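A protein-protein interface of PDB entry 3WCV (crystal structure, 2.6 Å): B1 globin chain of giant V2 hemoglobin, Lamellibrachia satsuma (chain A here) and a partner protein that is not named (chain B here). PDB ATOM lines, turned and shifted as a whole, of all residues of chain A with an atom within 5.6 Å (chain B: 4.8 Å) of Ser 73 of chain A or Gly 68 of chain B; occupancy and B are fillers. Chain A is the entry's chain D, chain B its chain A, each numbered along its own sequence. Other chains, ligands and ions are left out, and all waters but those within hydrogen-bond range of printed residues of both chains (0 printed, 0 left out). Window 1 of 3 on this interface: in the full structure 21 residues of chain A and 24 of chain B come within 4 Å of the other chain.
The side-chain sulfur (SD) of Met 77 of chain A sits close to the backbone NH (N) of Arg 65 of chain B (3.8 Å).
The backbone carbonyl oxygen (O) of Gly 68 of chain B is in hydrogen-bond range of the side-chain hydroxyl (OG) of Ser 73 of chain A, at 3.4 Å.
The side-chain sulfur (SD) of Met 77 of chain A lies close to the backbone carbonyl oxygen (O) of Ala 64 of chain B, at 3.4 Å.
Among the printed residues, pairs that only touch across the chains: Val 69 of chain A with Arg 72 of chain B (3.7 Å), Arg 70 of chain A with Arg 72 of chain B (3.7 Å) and Tyr 20 of chain A with Asp 71 of chain B (3.96 Å).
Ser 73 of chain A touches one residue of chain B.
Of chain A, only Ser 73 comes within 4 Å of Gly 68 of chain B.
Of the printed residues of chain A, Asp 71 of chain B touches Tyr 20 (3.96 Å).
Of the printed residues of chain A, Ala 64 of chain B touches Met 77 (3.4 Å).
The nearest residue of chain A that does not touch Gly 68 of chain B is Met 77 of chain A (5.1 Å).
Along chain A the printed residues that touch a printed residue of chain B span positions 20 to 77.
Of the 11 printed residues of chain B, 5 touch a printed residue of chain A.
Printed residues of chain B that touch a printed residue of chain A: Ala 64, Arg 65, Gly 68, Asp 71 and Arg 72.
Along chain B the printed residues that touch a printed residue of chain A span positions 64 to 72.
Among the printed residues, no Asp or Glu carboxylate lies within 4 Å of a Lys or Arg side-chain nitrogen of the other chain.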
ATOM      1  N   TYR A  20      34.342  15.810   6.688  1.00  0.00           N
ATOM      2  CA  TYR A  20      33.143  15.448   5.923  1.00  0.00           C
ATOM      3  C   TYR A  20      32.836  13.988   5.957  1.00  0.00           C
ATOM      4  O   TYR A  20      33.707  13.147   5.593  1.00  0.00           O
ATOM      5  CB  TYR A  20      33.271  15.932   4.471  1.00  0.00           C
ATOM      6  CG  TYR A  20      32.030  15.724   3.619  1.00  0.00           C
ATOM      7  CD1 TYR A  20      31.634  14.452   3.209  1.00  0.00           C
ATOM      8  CD2 TYR A  20      31.249  16.806   3.224  1.00  0.00           C
ATOM      9  CE1 TYR A  20      30.481  14.264   2.424  1.00  0.00           C
ATOM     10  CE2 TYR A  20      30.099  16.630   2.441  1.00  0.00           C
ATOM     11  CZ  TYR A  20      29.720  15.360   2.045  1.00  0.00           C
ATOM     12  OH  TYR A  20      28.598  15.185   1.256  1.00  0.00           O
ATOM     13  N   THR A  68      25.786  24.006  -2.981  1.00  0.00           N
ATOM     14  CA  THR A  68      27.066  23.693  -2.368  1.00  0.00           C
ATOM     15  C   THR A  68      27.037  22.270  -1.790  1.00  0.00           C
ATOM     16  O   THR A  68      28.017  21.523  -1.884  1.00  0.00           O
ATOM     17  CB  THR A  68      27.396  24.668  -1.220  1.00  0.00           C
ATOM     18  OG1 THR A  68      26.302  24.699  -0.293  1.00  0.00           O
ATOM     19  CG2 THR A  68      27.666  26.042  -1.752  1.00  0.00           C
ATOM     20  N   VAL A  69      25.923  21.908  -1.154  1.00  0.00           N
ATOM     21  CA  VAL A  69      25.782  20.563  -0.601  1.00  0.00           C
ATOM     22  C   VAL A  69      26.074  19.596  -1.745  1.00  0.00           C
ATOM     23  O   VAL A  69      26.886  18.678  -1.630  1.00  0.00           O
ATOM     24  CB  VAL A  69      24.345  20.331  -0.070  1.00  0.00           C
ATOM     25  CG1 VAL A  69      24.062  18.826   0.035  1.00  0.00           C
ATOM     26  CG2 VAL A  69      24.162  20.996   1.280  1.00  0.00           C
ATOM     27  N   ARG A  70      25.410  19.835  -2.866  1.00  0.00           N
ATOM     28  CA  ARG A  70      25.539  19.005  -4.060  1.00  0.00           C
ATOM     29  C   ARG A  70      26.992  18.932  -4.535  1.00  0.00           C
ATOM     30  O   ARG A  70      27.513  17.866  -4.880  1.00  0.00           O
ATOM     31  CB  ARG A  70      24.664  19.622  -5.145  1.00  0.00           C
ATOM     32  CG  ARG A  70      23.990  18.663  -6.087  1.00  0.00           C
ATOM     33  CD  ARG A  70      22.954  19.437  -6.896  1.00  0.00           C
ATOM     34  NE  ARG A  70      21.799  19.788  -6.076  1.00  0.00           N
ATOM     35  CZ  ARG A  70      21.222  20.984  -6.074  1.00  0.00           C
ATOM     36  NH1 ARG A  70      21.700  21.950  -6.852  1.00  0.00           N
ATOM     37  NH2 ARG A  70      20.160  21.206  -5.305  1.00  0.00           N
ATOM     38  N   VAL A  71      27.638  20.090  -4.545  1.00  0.00           N
ATOM     39  CA  VAL A  71      29.023  20.193  -4.991  1.00  0.00           C
ATOM     40  C   VAL A  71      29.989  19.409  -4.097  1.00  0.00           C
ATOM     41  O   VAL A  71      30.870  18.684  -4.589  1.00  0.00           O
ATOM     42  CB  VAL A  71      29.453  21.680  -5.059  1.00  0.00           C
ATOM     43  CG1 VAL A  71      30.935  21.780  -5.341  1.00  0.00           C
ATOM     44  CG2 VAL A  71      28.669  22.391  -6.164  1.00  0.00           C
ATOM     45  N   LEU A  72      29.811  19.552  -2.787  1.00  0.00           N
ATOM     46  CA  LEU A  72      30.655  18.841  -1.847  1.00  0.00           C
ATOM     47  C   LEU A  72      30.394  17.340  -1.892  1.00  0.00           C
ATOM     48  O   LEU A  72      31.334  16.562  -1.752  1.00  0.00           O
ATOM     49  CB  LEU A  72      30.443  19.385  -0.438  1.00  0.00           C
ATOM     50  CG  LEU A  72      30.925  20.826  -0.306  1.00  0.00           C
ATOM     51  CD1 LEU A  72      30.638  21.331   1.088  1.00  0.00           C
ATOM     52  CD2 LEU A  72      32.414  20.908  -0.627  1.00  0.00           C
ATOM     53  N   SER A  73      29.139  16.934  -2.087  1.00  0.00           N
ATOM     54  CA  SER A  73      28.809  15.515  -2.166  1.00  0.00           C
ATOM     55  C   SER A  73      29.529  14.920  -3.382  1.00  0.00           C
ATOM     56  O   SER A  73      29.997  13.780  -3.352  1.00  0.00           O
ATOM     57  CB  SER A  73      27.289  15.340  -2.290  1.00  0.00           C
ATOM     58  OG  SER A  73      26.927  13.999  -2.603  1.00  0.00           O
ATOM     59  N   GLY A  74      29.616  15.707  -4.451  1.00  0.00           N
ATOM     60  CA  GLY A  74      30.287  15.254  -5.663  1.00  0.00           C
ATOM     61  C   GLY A  74      31.772  15.081  -5.380  1.00  0.00           C
ATOM     62  O   GLY A  74      32.397  14.061  -5.718  1.00  0.00           O
ATOM     63  N   LEU A  75      32.337  16.096  -4.745  1.00  0.00           N
ATOM     64  CA  LEU A  75      33.735  16.065  -4.383  1.00  0.00           C
ATOM     65  C   LEU A  75      33.992  14.838  -3.495  1.00  0.00           C
ATOM     66  O   LEU A  75      34.990  14.143  -3.674  1.00  0.00           O
ATOM     67  CB  LEU A  75      34.105  17.346  -3.643  1.00  0.00           C
ATOM     68  CG  LEU A  75      35.526  17.441  -3.106  1.00  0.00           C
ATOM     69  CD1 LEU A  75      36.506  17.043  -4.188  1.00  0.00           C
ATOM     70  CD2 LEU A  75      35.793  18.867  -2.642  1.00  0.00           C
ATOM     71  N   ASP A  76      33.078  14.579  -2.559  1.00  0.00           N
ATOM     72  CA  ASP A  76      33.176  13.461  -1.633  1.00  0.00           C
ATOM     73  C   ASP A  76      33.117  12.152  -2.402  1.00  0.00           C
ATOM     74  O   ASP A  76      33.920  11.248  -2.181  1.00  0.00           O
ATOM     75  CB  ASP A  76      32.038  13.522  -0.616  1.00  0.00           C
ATOM     76  CG  ASP A  76      31.941  12.267   0.224  1.00  0.00           C
ATOM     77  OD1 ASP A  76      31.172  11.357  -0.142  1.00  0.00           O
ATOM     78  OD2 ASP A  76      32.629  12.181   1.257  1.00  0.00           O
ATOM     79  N   MET A  77      32.164  12.073  -3.319  1.00  0.00           N
ATOM     80  CA  MET A  77      31.992  10.898  -4.145  1.00  0.00           C
ATOM     81  C   MET A  77      33.275  10.620  -4.943  1.00  0.00           C
ATOM     82  O   MET A  77      33.653   9.468  -5.115  1.00  0.00           O
ATOM     83  CB  MET A  77      30.815  11.150  -5.065  1.00  0.00           C
ATOM     84  CG  MET A  77      30.359  10.003  -5.921  1.00  0.00           C
ATOM     85  SD  MET A  77      28.776  10.513  -6.581  1.00  0.00           S
ATOM     86  CE  MET A  77      29.342  11.637  -7.959  1.00  0.00           C
ATOM     87  N   GLY A  78      33.936  11.673  -5.424  1.00  0.00           N
ATOM     88  CA  GLY A  78      35.167  11.492  -6.174  1.00  0.00           C
ATOM     89  C   GLY A  78      36.329  10.998  -5.316  1.00  0.00           C
ATOM     90  O   GLY A  78      37.088  10.097  -5.693  1.00  0.00           O
ATOM     91  N   TYR B  18      25.853   3.180   6.189  1.00  0.00           N
ATOM     92  CA  TYR B  18      26.506   3.668   4.976  1.00  0.00           C
ATOM     93  C   TYR B  18      28.029   3.518   5.031  1.00  0.00           C
ATOM     94  O   TYR B  18      28.660   3.171   4.037  1.00  0.00           O
ATOM     95  CB  TYR B  18      26.117   5.126   4.789  1.00  0.00           C
ATOM     96  CG  TYR B  18      26.671   5.802   3.574  1.00  0.00           C
ATOM     97  CD1 TYR B  18      26.419   5.293   2.304  1.00  0.00           C
ATOM     98  CD2 TYR B  18      27.356   7.024   3.680  1.00  0.00           C
ATOM     99  CE1 TYR B  18      26.818   5.975   1.163  1.00  0.00           C
ATOM    100  CE2 TYR B  18      27.764   7.719   2.543  1.00  0.00           C
ATOM    101  CZ  TYR B  18      27.483   7.186   1.285  1.00  0.00           C
ATOM    102  OH  TYR B  18      27.844   7.881   0.148  1.00  0.00           O
ATOM    103  N   ILE B  63      25.412   3.884  -9.142  1.00  0.00           N
ATOM    104  CA  ILE B  63      25.209   3.492  -7.754  1.00  0.00           C
ATOM    105  C   ILE B  63      25.789   4.575  -6.840  1.00  0.00           C
ATOM    106  O   ILE B  63      25.127   5.025  -5.902  1.00  0.00           O
ATOM    107  CB  ILE B  63      25.900   2.149  -7.454  1.00  0.00           C
ATOM    108  CG1 ILE B  63      25.194   1.038  -8.236  1.00  0.00           C
ATOM    109  CG2 ILE B  63      25.881   1.868  -5.953  1.00  0.00           C
ATOM    110  CD1 ILE B  63      25.780  -0.324  -8.051  1.00  0.00           C
ATOM    111  N   ALA B  64      27.007   5.013  -7.148  1.00  0.00           N
ATOM    112  CA  ALA B  64      27.683   6.032  -6.349  1.00  0.00           C
ATOM    113  C   ALA B  64      26.909   7.352  -6.339  1.00  0.00           C
ATOM    114  O   ALA B  64      26.797   8.003  -5.287  1.00  0.00           O
ATOM    115  CB  ALA B  64      29.133   6.261  -6.869  1.00  0.00           C
ATOM    116  N   ARG B  65      26.358   7.733  -7.490  1.00  0.00           N
ATOM    117  CA  ARG B  65      25.615   8.981  -7.547  1.00  0.00           C
ATOM    118  C   ARG B  65      24.343   8.906  -6.718  1.00  0.00           C
ATOM    119  O   ARG B  65      24.006   9.849  -5.993  1.00  0.00           O
ATOM    120  CB  ARG B  65      25.283   9.363  -8.996  1.00  0.00           C
ATOM    121  CG  ARG B  65      26.441  10.067  -9.704  1.00  0.00           C
ATOM    122  CD  ARG B  65      26.045  10.642 -11.056  1.00  0.00           C
ATOM    123  NE  ARG B  65      25.643   9.619 -12.043  1.00  0.00           N
ATOM    124  CZ  ARG B  65      26.472   8.933 -12.839  1.00  0.00           C
ATOM    125  NH1 ARG B  65      27.785   9.130 -12.791  1.00  0.00           N
ATOM    126  NH2 ARG B  65      25.987   8.066 -13.716  1.00  0.00           N
ATOM    127  N   VAL B  66      23.657   7.776  -6.811  1.00  0.00           N
ATOM    128  CA  VAL B  66      22.414   7.564  -6.089  1.00  0.00           C
ATOM    129  C   VAL B  66      22.567   7.537  -4.571  1.00  0.00           C
ATOM    130  O   VAL B  66      21.775   8.147  -3.869  1.00  0.00           O
ATOM    131  CB  VAL B  66      21.743   6.251  -6.530  1.00  0.00           C
ATOM    132  CG1 VAL B  66      20.530   5.965  -5.672  1.00  0.00           C
ATOM    133  CG2 VAL B  66      21.363   6.330  -7.990  1.00  0.00           C
ATOM    134  N   ILE B  67      23.554   6.818  -4.045  1.00  0.00           N
ATOM    135  CA  ILE B  67      23.703   6.778  -2.600  1.00  0.00           C
ATOM    136  C   ILE B  67      24.280   8.100  -2.144  1.00  0.00           C
ATOM    137  O   ILE B  67      24.049   8.536  -1.017  1.00  0.00           O
ATOM    138  CB  ILE B  67      24.596   5.599  -2.133  1.00  0.00           C
ATOM    139  CG1 ILE B  67      25.977   5.694  -2.779  1.00  0.00           C
ATOM    140  CG2 ILE B  67      23.910   4.255  -2.490  1.00  0.00           C
ATOM    141  CD1 ILE B  67      26.900   4.609  -2.335  1.00  0.00           C
ATOM    142  N   GLY B  68      25.024   8.757  -3.018  1.00  0.00           N
ATOM    143  CA  GLY B  68      25.565  10.051  -2.645  1.00  0.00           C
ATOM    144  C   GLY B  68      24.392  11.011  -2.476  1.00  0.00           C
ATOM    145  O   GLY B  68      24.397  11.896  -1.594  1.00  0.00           O
ATOM    146  N   GLY B  69      23.377  10.818  -3.324  1.00  0.00           N
ATOM    147  CA  GLY B  69      22.177  11.637  -3.294  1.00  0.00           C
ATOM    148  C   GLY B  69      21.384  11.351  -2.038  1.00  0.00           C
ATOM    149  O   GLY B  69      20.940  12.276  -1.351  1.00  0.00           O
ATOM    150  N   LEU B  70      21.179  10.075  -1.735  1.00  0.00           N
ATOM    151  CA  LEU B  70      20.482   9.718  -0.508  1.00  0.00           C
ATOM    152  C   LEU B  70      21.234  10.380   0.652  1.00  0.00           C
ATOM    153  O   LEU B  70      20.626  11.010   1.519  1.00  0.00           O
ATOM    154  CB  LEU B  70      20.502   8.207  -0.317  1.00  0.00           C
ATOM    155  CG  LEU B  70      19.383   7.464  -1.035  1.00  0.00           C
ATOM    156  CD1 LEU B  70      19.679   5.957  -1.123  1.00  0.00           C
ATOM    157  CD2 LEU B  70      18.071   7.749  -0.275  1.00  0.00           C
ATOM    158  N   ASP B  71      22.559  10.252   0.659  1.00  0.00           N
ATOM    159  CA  ASP B  71      23.370  10.838   1.727  1.00  0.00           C
ATOM    160  C   ASP B  71      23.257  12.354   1.904  1.00  0.00           C
ATOM    161  O   ASP B  71      23.102  12.841   3.027  1.00  0.00           O
ATOM    162  CB  ASP B  71      24.847  10.483   1.562  1.00  0.00           C
ATOM    163  CG  ASP B  71      25.709  11.077   2.677  1.00  0.00           C
ATOM    164  OD1 ASP B  71      25.724  10.471   3.783  1.00  0.00           O
ATOM    165  OD2 ASP B  71      26.342  12.155   2.458  1.00  0.00           O
ATOM    166  N   ARG B  72      23.361  13.109   0.817  1.00  0.00           N
ATOM    167  CA  ARG B  72      23.257  14.569   0.920  1.00  0.00           C
ATOM    168  C   ARG B  72      21.836  14.977   1.303  1.00  0.00           C
ATOM    169  O   ARG B  72      21.636  15.970   2.016  1.00  0.00           O
ATOM    170  CB  ARG B  72      23.638  15.215  -0.396  1.00  0.00           C
ATOM    171  CG  ARG B  72      22.643  14.978  -1.481  1.00  0.00           C
ATOM    172  CD  ARG B  72      23.174  15.510  -2.779  1.00  0.00           C
ATOM    173  NE  ARG B  72      22.074  15.951  -3.618  1.00  0.00           N
ATOM    174  CZ  ARG B  72      22.025  15.772  -4.923  1.00  0.00           C
ATOM    175  NH1 ARG B  72      23.022  15.165  -5.528  1.00  0.00           N
ATOM    176  NH2 ARG B  72      20.975  16.180  -5.606  1.00  0.00           N
